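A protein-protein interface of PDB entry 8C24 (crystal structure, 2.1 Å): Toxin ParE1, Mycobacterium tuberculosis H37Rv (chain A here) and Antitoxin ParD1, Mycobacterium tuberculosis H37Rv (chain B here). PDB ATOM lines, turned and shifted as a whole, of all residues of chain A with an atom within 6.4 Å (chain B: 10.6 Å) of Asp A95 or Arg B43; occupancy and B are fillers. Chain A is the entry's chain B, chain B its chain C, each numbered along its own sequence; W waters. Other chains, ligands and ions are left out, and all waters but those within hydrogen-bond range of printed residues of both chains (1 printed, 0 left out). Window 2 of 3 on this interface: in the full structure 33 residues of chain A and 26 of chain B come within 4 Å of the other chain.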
ATOM      1  N   ARG A  53      30.214  24.267 -25.404  1.00  0.00           N
ATOM      2  CA  ARG A  53      28.788  24.620 -25.422  1.00  0.00           C
ATOM      3  C   ARG A  53      28.126  23.958 -24.220  1.00  0.00           C
ATOM      4  O   ARG A  53      28.298  22.772 -24.027  1.00  0.00           O
ATOM      5  CB  ARG A  53      28.175  24.167 -26.745  1.00  0.00           C
ATOM      6  CG  ARG A  53      26.656  24.159 -26.759  1.00  0.00           C
ATOM      7  CD  ARG A  53      26.103  23.295 -27.875  1.00  0.00           C
ATOM      8  NE  ARG A  53      26.435  23.806 -29.196  1.00  0.00           N
ATOM      9  CZ  ARG A  53      25.608  23.802 -30.231  1.00  0.00           C
ATOM     10  NH1 ARG A  53      24.391  23.305 -30.103  1.00  0.00           N
ATOM     11  NH2 ARG A  53      25.995  24.299 -31.393  1.00  0.00           N
ATOM     12  N   GLU A  57      20.608  20.162 -21.369  1.00  0.00           N
ATOM     13  CA  GLU A  57      19.540  19.305 -21.868  1.00  0.00           C
ATOM     14  C   GLU A  57      20.000  17.860 -22.029  1.00  0.00           C
ATOM     15  O   GLU A  57      19.164  16.949 -22.005  1.00  0.00           O
ATOM     16  CB  GLU A  57      18.972  19.868 -23.186  1.00  0.00           C
ATOM     17  CG  GLU A  57      19.873  19.769 -24.425  1.00  0.00           C
ATOM     18  CD  GLU A  57      20.975  20.841 -24.497  1.00  0.00           C
ATOM     19  OE1 GLU A  57      21.098  21.618 -23.515  1.00  0.00           O
ATOM     20  OE2 GLU A  57      21.713  20.905 -25.516  1.00  0.00           O
ATOM     21  N   ILE A  58      21.306  17.623 -22.175  1.00  0.00           N
ATOM     22  CA  ILE A  58      21.813  16.259 -22.051  1.00  0.00           C
ATOM     23  C   ILE A  58      21.898  15.858 -20.583  1.00  0.00           C
ATOM     24  O   ILE A  58      21.363  14.824 -20.168  1.00  0.00           O
ATOM     25  CB  ILE A  58      23.182  16.106 -22.749  1.00  0.00           C
ATOM     26  CG1 ILE A  58      23.033  16.218 -24.268  1.00  0.00           C
ATOM     27  CG2 ILE A  58      23.810  14.745 -22.392  1.00  0.00           C
ATOM     28  CD1 ILE A  58      23.247  17.599 -24.823  1.00  0.00           C
ATOM     29  N   LYS A  64      30.261  20.657 -23.601  1.00  0.00           N
ATOM     30  CA  LYS A  64      30.832  19.742 -24.573  1.00  0.00           C
ATOM     31  C   LYS A  64      31.709  20.528 -25.539  1.00  0.00           C
ATOM     32  O   LYS A  64      31.439  21.692 -25.835  1.00  0.00           O
ATOM     33  CB  LYS A  64      29.734  18.960 -25.336  1.00  0.00           C
ATOM     34  CG  LYS A  64      28.470  19.783 -25.638  1.00  0.00           C
ATOM     35  CD  LYS A  64      27.514  19.045 -26.575  1.00  0.00           C
ATOM     36  CE  LYS A  64      28.264  18.529 -27.789  1.00  0.00           C
ATOM     37  NZ  LYS A  64      27.369  18.336 -28.964  1.00  0.00           N
ATOM     38  N   GLN A  90      32.787  10.901 -31.997  1.00  0.00           N
ATOM     39  CA  GLN A  90      31.863  11.851 -32.613  1.00  0.00           C
ATOM     40  C   GLN A  90      30.580  11.183 -33.095  1.00  0.00           C
ATOM     41  O   GLN A  90      29.542  11.846 -33.175  1.00  0.00           O
ATOM     42  CB  GLN A  90      32.554  12.584 -33.783  1.00  0.00           C
ATOM     43  CG  GLN A  90      32.945  11.713 -34.983  1.00  0.00           C
ATOM     44  CD  GLN A  90      33.904  12.422 -35.974  1.00  0.00           C
ATOM     45  OE1 GLN A  90      34.024  13.642 -35.973  1.00  0.00           O
ATOM     46  NE2 GLN A  90      34.580  11.644 -36.811  1.00  0.00           N
ATOM     47  N   MET A  92      28.600   9.543 -31.554  1.00  0.00           N
ATOM     48  CA  MET A  92      27.576   9.705 -30.535  1.00  0.00           C
ATOM     49  C   MET A  92      27.152  11.146 -30.345  1.00  0.00           C
ATOM     50  O   MET A  92      26.171  11.393 -29.636  1.00  0.00           O
ATOM     51  CB  MET A  92      28.065   9.175 -29.194  1.00  0.00           C
ATOM     52  CG  MET A  92      28.420   7.722 -29.196  1.00  0.00           C
ATOM     53  SD  MET A  92      28.903   7.294 -27.524  1.00  0.00           S
ATOM     54  CE  MET A  92      27.324   7.418 -26.662  1.00  0.00           C
ATOM     55  N   ASP A  93      27.870  12.099 -30.932  1.00  0.00           N
ATOM     56  CA  ASP A  93      27.555  13.501 -30.705  1.00  0.00           C
ATOM     57  C   ASP A  93      26.271  13.862 -31.448  1.00  0.00           C
ATOM     58  O   ASP A  93      26.189  13.712 -32.672  1.00  0.00           O
ATOM     59  CB  ASP A  93      28.711  14.390 -31.157  1.00  0.00           C
ATOM     60  CG  ASP A  93      28.579  15.809 -30.644  1.00  0.00           C
ATOM     61  OD1 ASP A  93      27.599  16.083 -29.907  1.00  0.00           O
ATOM     62  OD2 ASP A  93      29.457  16.643 -30.961  1.00  0.00           O
ATOM     63  N   VAL A  94      25.317  14.396 -30.704  1.00  0.00           N
ATOM     64  CA  VAL A  94      23.973  14.693 -31.256  1.00  0.00           C
ATOM     65  C   VAL A  94      23.914  16.049 -31.961  1.00  0.00           C
ATOM     66  O   VAL A  94      23.082  16.149 -32.855  1.00  0.00           O
ATOM     67  CB  VAL A  94      22.928  14.624 -30.134  1.00  0.00           C
ATOM     68  CG1 VAL A  94      23.242  15.625 -29.045  1.00  0.00           C
ATOM     69  CG2 VAL A  94      21.539  14.871 -30.674  1.00  0.00           C
ATOM     70  N   ASP A  95      24.761  17.008 -31.564  1.00  0.00           N
ATOM     71  CA  ASP A  95      24.796  18.434 -32.009  1.00  0.00           C
ATOM     72  C   ASP A  95      23.615  19.176 -31.375  1.00  0.00           C
ATOM     73  O   ASP A  95      22.475  18.924 -31.801  1.00  0.00           O
ATOM     74  CB  ASP A  95      24.877  18.696 -33.517  1.00  0.00           C
ATOM     75  CG  ASP A  95      26.063  18.071 -34.215  1.00  0.00           C
ATOM     76  OD1 ASP A  95      26.197  16.855 -34.153  1.00  0.00           O
ATOM     77  OD2 ASP A  95      26.817  18.812 -34.848  1.00  0.00           O
ATOM     78  N   SER B  35       5.713  14.079 -38.097  1.00  0.00           N
ATOM     79  CA  SER B  35       7.113  14.096 -38.499  1.00  0.00           C
ATOM     80  C   SER B  35       7.991  14.670 -37.383  1.00  0.00           C
ATOM     81  O   SER B  35       8.984  14.060 -36.992  1.00  0.00           O
ATOM     82  CB  SER B  35       7.270  14.883 -39.803  1.00  0.00           C
ATOM     83  OG  SER B  35       8.640  14.998 -40.156  1.00  0.00           O
ATOM     84  N   ALA B  36       7.601  15.817 -36.808  1.00  0.00           N
ATOM     85  CA  ALA B  36       8.392  16.423 -35.733  1.00  0.00           C
ATOM     86  C   ALA B  36       8.540  15.492 -34.536  1.00  0.00           C
ATOM     87  O   ALA B  36       9.604  15.451 -33.905  1.00  0.00           O
ATOM     88  CB  ALA B  36       7.763  17.747 -35.290  1.00  0.00           C
ATOM     89  N   LEU B  37       7.490  14.736 -34.199  1.00  0.00           N
ATOM     90  CA  LEU B  37       7.584  13.856 -33.036  1.00  0.00           C
ATOM     91  C   LEU B  37       8.472  12.639 -33.310  1.00  0.00           C
ATOM     92  O   LEU B  37       9.133  12.134 -32.387  1.00  0.00           O
ATOM     93  CB  LEU B  37       6.173  13.426 -32.588  1.00  0.00           C
ATOM     94  CG  LEU B  37       5.315  14.527 -31.919  1.00  0.00           C
ATOM     95  CD1 LEU B  37       3.807  14.144 -31.866  1.00  0.00           C
ATOM     96  CD2 LEU B  37       5.796  14.853 -30.518  1.00  0.00           C
ATOM     97  N   ARG B  38       8.511  12.156 -34.560  1.00  0.00           N
ATOM     98  CA  ARG B  38       9.481  11.116 -34.908  1.00  0.00           C
ATOM     99  C   ARG B  38      10.923  11.628 -34.802  1.00  0.00           C
ATOM    100  O   ARG B  38      11.806  10.901 -34.339  1.00  0.00           O
ATOM    101  CB  ARG B  38       9.214  10.594 -36.307  1.00  0.00           C
ATOM    102  CG  ARG B  38       7.846   9.925 -36.457  1.00  0.00           C
ATOM    103  CD  ARG B  38       7.803   9.160 -37.748  1.00  0.00           C
ATOM    104  NE  ARG B  38       7.918  10.049 -38.893  1.00  0.00           N
ATOM    105  CZ  ARG B  38       6.874  10.599 -39.497  1.00  0.00           C
ATOM    106  NH1 ARG B  38       5.660  10.358 -39.027  1.00  0.00           N
ATOM    107  NH2 ARG B  38       7.039  11.387 -40.555  1.00  0.00           N
ATOM    108  N   LEU B  39      11.130  12.885 -35.151  1.00  0.00           N
ATOM    109  CA  LEU B  39      12.452  13.531 -35.037  1.00  0.00           C
ATOM    110  C   LEU B  39      12.824  13.617 -33.559  1.00  0.00           C
ATOM    111  O   LEU B  39      13.953  13.338 -33.226  1.00  0.00           O
ATOM    112  CB  LEU B  39      12.324  14.937 -35.605  1.00  0.00           C
ATOM    113  CG  LEU B  39      13.258  15.257 -36.756  1.00  0.00           C
ATOM    114  CD1 LEU B  39      12.716  14.709 -38.058  1.00  0.00           C
ATOM    115  CD2 LEU B  39      13.490  16.747 -36.841  1.00  0.00           C
ATOM    116  N   LEU B  40      11.867  13.985 -32.719  1.00  0.00           N
ATOM    117  CA  LEU B  40      12.135  14.126 -31.291  1.00  0.00           C
ATOM    118  C   LEU B  40      12.499  12.785 -30.679  1.00  0.00           C
ATOM    119  O   LEU B  40      13.456  12.684 -29.902  1.00  0.00           O
ATOM    120  CB  LEU B  40      10.929  14.731 -30.577  1.00  0.00           C
ATOM    121  CG  LEU B  40      11.171  15.125 -29.111  1.00  0.00           C
ATOM    122  CD1 LEU B  40      12.112  16.336 -28.989  1.00  0.00           C
ATOM    123  CD2 LEU B  40       9.862  15.399 -28.405  1.00  0.00           C
ATOM    124  N   GLU B  41      11.754  11.734 -31.029  1.00  0.00           N
ATOM    125  CA  GLU B  41      12.046  10.408 -30.487  1.00  0.00           C
ATOM    126  C   GLU B  41      13.413   9.911 -30.940  1.00  0.00           C
ATOM    127  O   GLU B  41      14.134   9.263 -30.165  1.00  0.00           O
ATOM    128  CB  GLU B  41      10.965   9.415 -30.906  1.00  0.00           C
ATOM    129  CG  GLU B  41      11.266   7.978 -30.541  1.00  0.00           C
ATOM    130  CD  GLU B  41      10.049   7.090 -30.749  1.00  0.00           C
ATOM    131  OE1 GLU B  41       9.520   7.077 -31.876  1.00  0.00           O
ATOM    132  OE2 GLU B  41       9.611   6.430 -29.784  1.00  0.00           O
ATOM    133  N   ASP B  42      13.776  10.187 -32.198  1.00  0.00           N
ATOM    134  CA  ASP B  42      15.099   9.818 -32.690  1.00  0.00           C
ATOM    135  C   ASP B  42      16.182  10.563 -31.915  1.00  0.00           C
ATOM    136  O   ASP B  42      17.178   9.965 -31.491  1.00  0.00           O
ATOM    137  CB  ASP B  42      15.203  10.103 -34.198  1.00  0.00           C
ATOM    138  CG  ASP B  42      14.362   9.126 -35.051  1.00  0.00           C
ATOM    139  OD1 ASP B  42      13.929   8.064 -34.520  1.00  0.00           O
ATOM    140  OD2 ASP B  42      14.116   9.430 -36.254  1.00  0.00           O
ATOM    141  N   ARG B  43      15.981  11.863 -31.691  1.00  0.00           N
ATOM    142  CA  ARG B  43      16.891  12.635 -30.856  1.00  0.00           C
ATOM    143  C   ARG B  43      16.991  12.032 -29.458  1.00  0.00           C
ATOM    144  O   ARG B  43      18.090  11.738 -28.974  1.00  0.00           O
ATOM    145  CB  ARG B  43      16.424  14.091 -30.783  1.00  0.00           C
ATOM    146  CG  ARG B  43      17.476  15.044 -30.191  1.00  0.00           C
ATOM    147  CD  ARG B  43      16.874  16.409 -29.835  1.00  0.00           C
ATOM    148  NE  ARG B  43      17.741  17.163 -28.927  1.00  0.00           N
ATOM    149  CZ  ARG B  43      18.824  17.834 -29.314  1.00  0.00           C
ATOM    150  NH1 ARG B  43      19.170  17.854 -30.592  1.00  0.00           N
ATOM    151  NH2 ARG B  43      19.561  18.484 -28.421  1.00  0.00           N
ATOM    152  N   GLU B  44      15.842  11.793 -28.816  1.00  0.00           N
ATOM    153  CA  GLU B  44      15.836  11.320 -27.439  1.00  0.00           C
ATOM    154  C   GLU B  44      16.579  10.013 -27.292  1.00  0.00           C
ATOM    155  O   GLU B  44      17.209   9.769 -26.257  1.00  0.00           O
ATOM    156  CB  GLU B  44      14.410  11.141 -26.934  1.00  0.00           C
ATOM    157  CG  GLU B  44      13.957  12.209 -25.977  1.00  0.00           C
ATOM    158  CD  GLU B  44      14.914  12.428 -24.826  1.00  0.00           C
ATOM    159  OE1 GLU B  44      15.460  11.443 -24.253  1.00  0.00           O
ATOM    160  OE2 GLU B  44      15.112  13.615 -24.498  1.00  0.00           O
ATOM    161  N   THR B  45      16.482   9.136 -28.292  1.00  0.00           N
ATOM    162  CA  THR B  45      17.217   7.877 -28.210  1.00  0.00           C
ATOM    163  C   THR B  45      18.725   8.125 -28.239  1.00  0.00           C
ATOM    164  O   THR B  45      19.477   7.498 -27.483  1.00  0.00           O
ATOM    165  CB  THR B  45      16.798   6.941 -29.346  1.00  0.00           C
ATOM    166  OG1 THR B  45      15.370   6.883 -29.413  1.00  0.00           O
ATOM    167  CG2 THR B  45      17.355   5.537 -29.121  1.00  0.00           C
ATOM    168  N   GLN B  46      19.184   9.046 -29.096  1.00  0.00           N
ATOM    169  CA  GLN B  46      20.592   9.419 -29.080  1.00  0.00           C
ATOM    170  C   GLN B  46      20.962  10.112 -27.778  1.00  0.00           C
ATOM    171  O   GLN B  46      22.037   9.856 -27.227  1.00  0.00           O
ATOM    172  CB  GLN B  46      20.922  10.308 -30.279  1.00  0.00           C
ATOM    173  CG  GLN B  46      20.734   9.607 -31.608  1.00  0.00           C
ATOM    174  CD  GLN B  46      20.657  10.584 -32.753  1.00  0.00           C
ATOM    175  OE1 GLN B  46      21.674  11.109 -33.213  1.00  0.00           O
ATOM    176  NE2 GLN B  46      19.446  10.856 -33.207  1.00  0.00           N
ATOM    177  N   LEU B  47      20.078  10.976 -27.255  1.00  0.00           N
ATOM    178  CA  LEU B  47      20.361  11.641 -25.985  1.00  0.00           C
ATOM    179  C   LEU B  47      20.438  10.639 -24.846  1.00  0.00           C
ATOM    180  O   LEU B  47      21.294  10.756 -23.957  1.00  0.00           O
ATOM    181  CB  LEU B  47      19.302  12.690 -25.669  1.00  0.00           C
ATOM    182  CG  LEU B  47      19.266  13.944 -26.527  1.00  0.00           C
ATOM    183  CD1 LEU B  47      18.050  14.788 -26.150  1.00  0.00           C
ATOM    184  CD2 LEU B  47      20.544  14.728 -26.336  1.00  0.00           C
ATOM    185  N   ARG B  48      19.546   9.648 -24.853  1.00  0.00           N
ATOM    186  CA  ARG B  48      19.617   8.585 -23.863  1.00  0.00           C
ATOM    187  C   ARG B  48      20.979   7.893 -23.891  1.00  0.00           C
ATOM    188  O   ARG B  48      21.560   7.607 -22.835  1.00  0.00           O
ATOM    189  CB  ARG B  48      18.498   7.575 -24.103  1.00  0.00           C
ATOM    190  CG  ARG B  48      18.633   6.340 -23.253  1.00  0.00           C
ATOM    191  CD  ARG B  48      17.337   5.547 -23.190  1.00  0.00           C
ATOM    192  NE  ARG B  48      17.528   4.349 -22.383  1.00  0.00           N
ATOM    193  CZ  ARG B  48      16.577   3.464 -22.104  1.00  0.00           C
ATOM    194  NH1 ARG B  48      15.348   3.632 -22.581  1.00  0.00           N
ATOM    195  NH2 ARG B  48      16.864   2.408 -21.348  1.00  0.00           N
ATOM    196  N   ALA B  49      21.513   7.626 -25.086  1.00  0.00           N
ATOM    197  CA  ALA B  49      22.820   6.971 -25.161  1.00  0.00           C
ATOM    198  C   ALA B  49      23.918   7.858 -24.575  1.00  0.00           C
ATOM    199  O   ALA B  49      24.828   7.362 -23.894  1.00  0.00           O
ATOM    200  CB  ALA B  49      23.154   6.585 -26.600  1.00  0.00           C
ATOM    201  N   LEU B  50      23.839   9.172 -24.805  1.00  0.00           N
ATOM    202  CA  LEU B  50      24.847  10.077 -24.259  1.00  0.00           C
ATOM    203  C   LEU B  50      24.743  10.169 -22.741  1.00  0.00           C
ATOM    204  O   LEU B  50      25.765  10.213 -22.048  1.00  0.00           O
ATOM    205  CB  LEU B  50      24.703  11.466 -24.864  1.00  0.00           C
ATOM    206  CG  LEU B  50      25.165  11.700 -26.295  1.00  0.00           C
ATOM    207  CD1 LEU B  50      24.954  13.176 -26.627  1.00  0.00           C
ATOM    208  CD2 LEU B  50      26.615  11.274 -26.480  1.00  0.00           C
ATOM    209  N   ARG B  51      23.517  10.225 -22.217  1.00  0.00           N
ATOM    210  CA  ARG B  51      23.316  10.349 -20.774  1.00  0.00           C
ATOM    211  C   ARG B  51      23.855   9.132 -20.051  1.00  0.00           C
ATOM    212  O   ARG B  51      24.596   9.252 -19.070  1.00  0.00           O
ATOM    213  CB  ARG B  51      21.835  10.529 -20.454  1.00  0.00           C
ATOM    214  CG  ARG B  51      21.245  11.801 -20.968  1.00  0.00           C
ATOM    215  CD  ARG B  51      19.827  12.037 -20.439  1.00  0.00           C
ATOM    216  NE  ARG B  51      19.283  13.237 -21.067  1.00  0.00           N
ATOM    217  CZ  ARG B  51      18.231  13.247 -21.878  1.00  0.00           C
ATOM    218  NH1 ARG B  51      17.580  12.113 -22.140  1.00  0.00           N
ATOM    219  NH2 ARG B  51      17.822  14.394 -22.414  1.00  0.00           N
HETATM  220  O   HOH W   1      24.197   9.391 -28.939  1.00  0.00           O
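Of the 9 printed residues of chain A, 5 touch a printed residue of chain B.
Hydrophobic or aromatic side chains of chain A that line the printed part of chain B: Ile A58, Met A92 and Val A94.
Hydrophobic or aromatic side chains of chain B that line the printed part of chain A: Leu B47 and Leu B50.
The side-chain carboxylate (OE1) of Glu B44 lies within salt-bridge range of the guanidinium group (NH1) of Arg B51.
The side-chain carboxylate (OD1) of Asp A93 lies within hydrogen-bond range of the backbone NH (N) of Asp A95, at 3.4 Å.
Water W1 lies within hydrogen-bond range of the backbone carbonyl oxygen of Gln B46 (2.8 Å) and the backbone carbonyl oxygen of Met A92 (2.9 Å).
The guanidinium group (NH2) of Arg B51 sits at hydrogen-bond distance from the backbone carbonyl oxygen (O) of Glu A57, 2.9 Å away.
The guanidinium group (NE) of Arg B51 lies within hydrogen-bond range of the backbone carbonyl oxygen (O) of Ile A58.
Among the printed residues, pairs that only touch across the chains: Met A92 with Leu B50 (3.2 Å), Ile A58 with Leu B47 (3.6 Å), Asp A95 with Arg B43 (3.7 Å), Met A92 with Ala B49 (3.7 Å), Val A94 with Arg B43 (3.8 Å), Val A94 with Leu B50 (3.8 Å) and Val A94 with Leu B47 (3.9 Å).
Of the printed residues of chain B, Ile A58 touches Leu B47 and Arg B51.
No residue of chain B comes within 4 Å of Asp A93.
Val A94 touches just these residues of chain B: Arg B43, Leu B47 and Leu B50.
Asp A95 touches just one residue of chain B: Arg B43 (3.7 Å).
Of the printed residues of chain A, Ala B49 touches Met A92 (3.7 Å).
The nearest residue of chain B that does not touch Asp A95 is Leu B50 (6.3 Å).
The nearest residue of chain A that does not touch Arg B43 is Glu A57 (4.2 Å).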
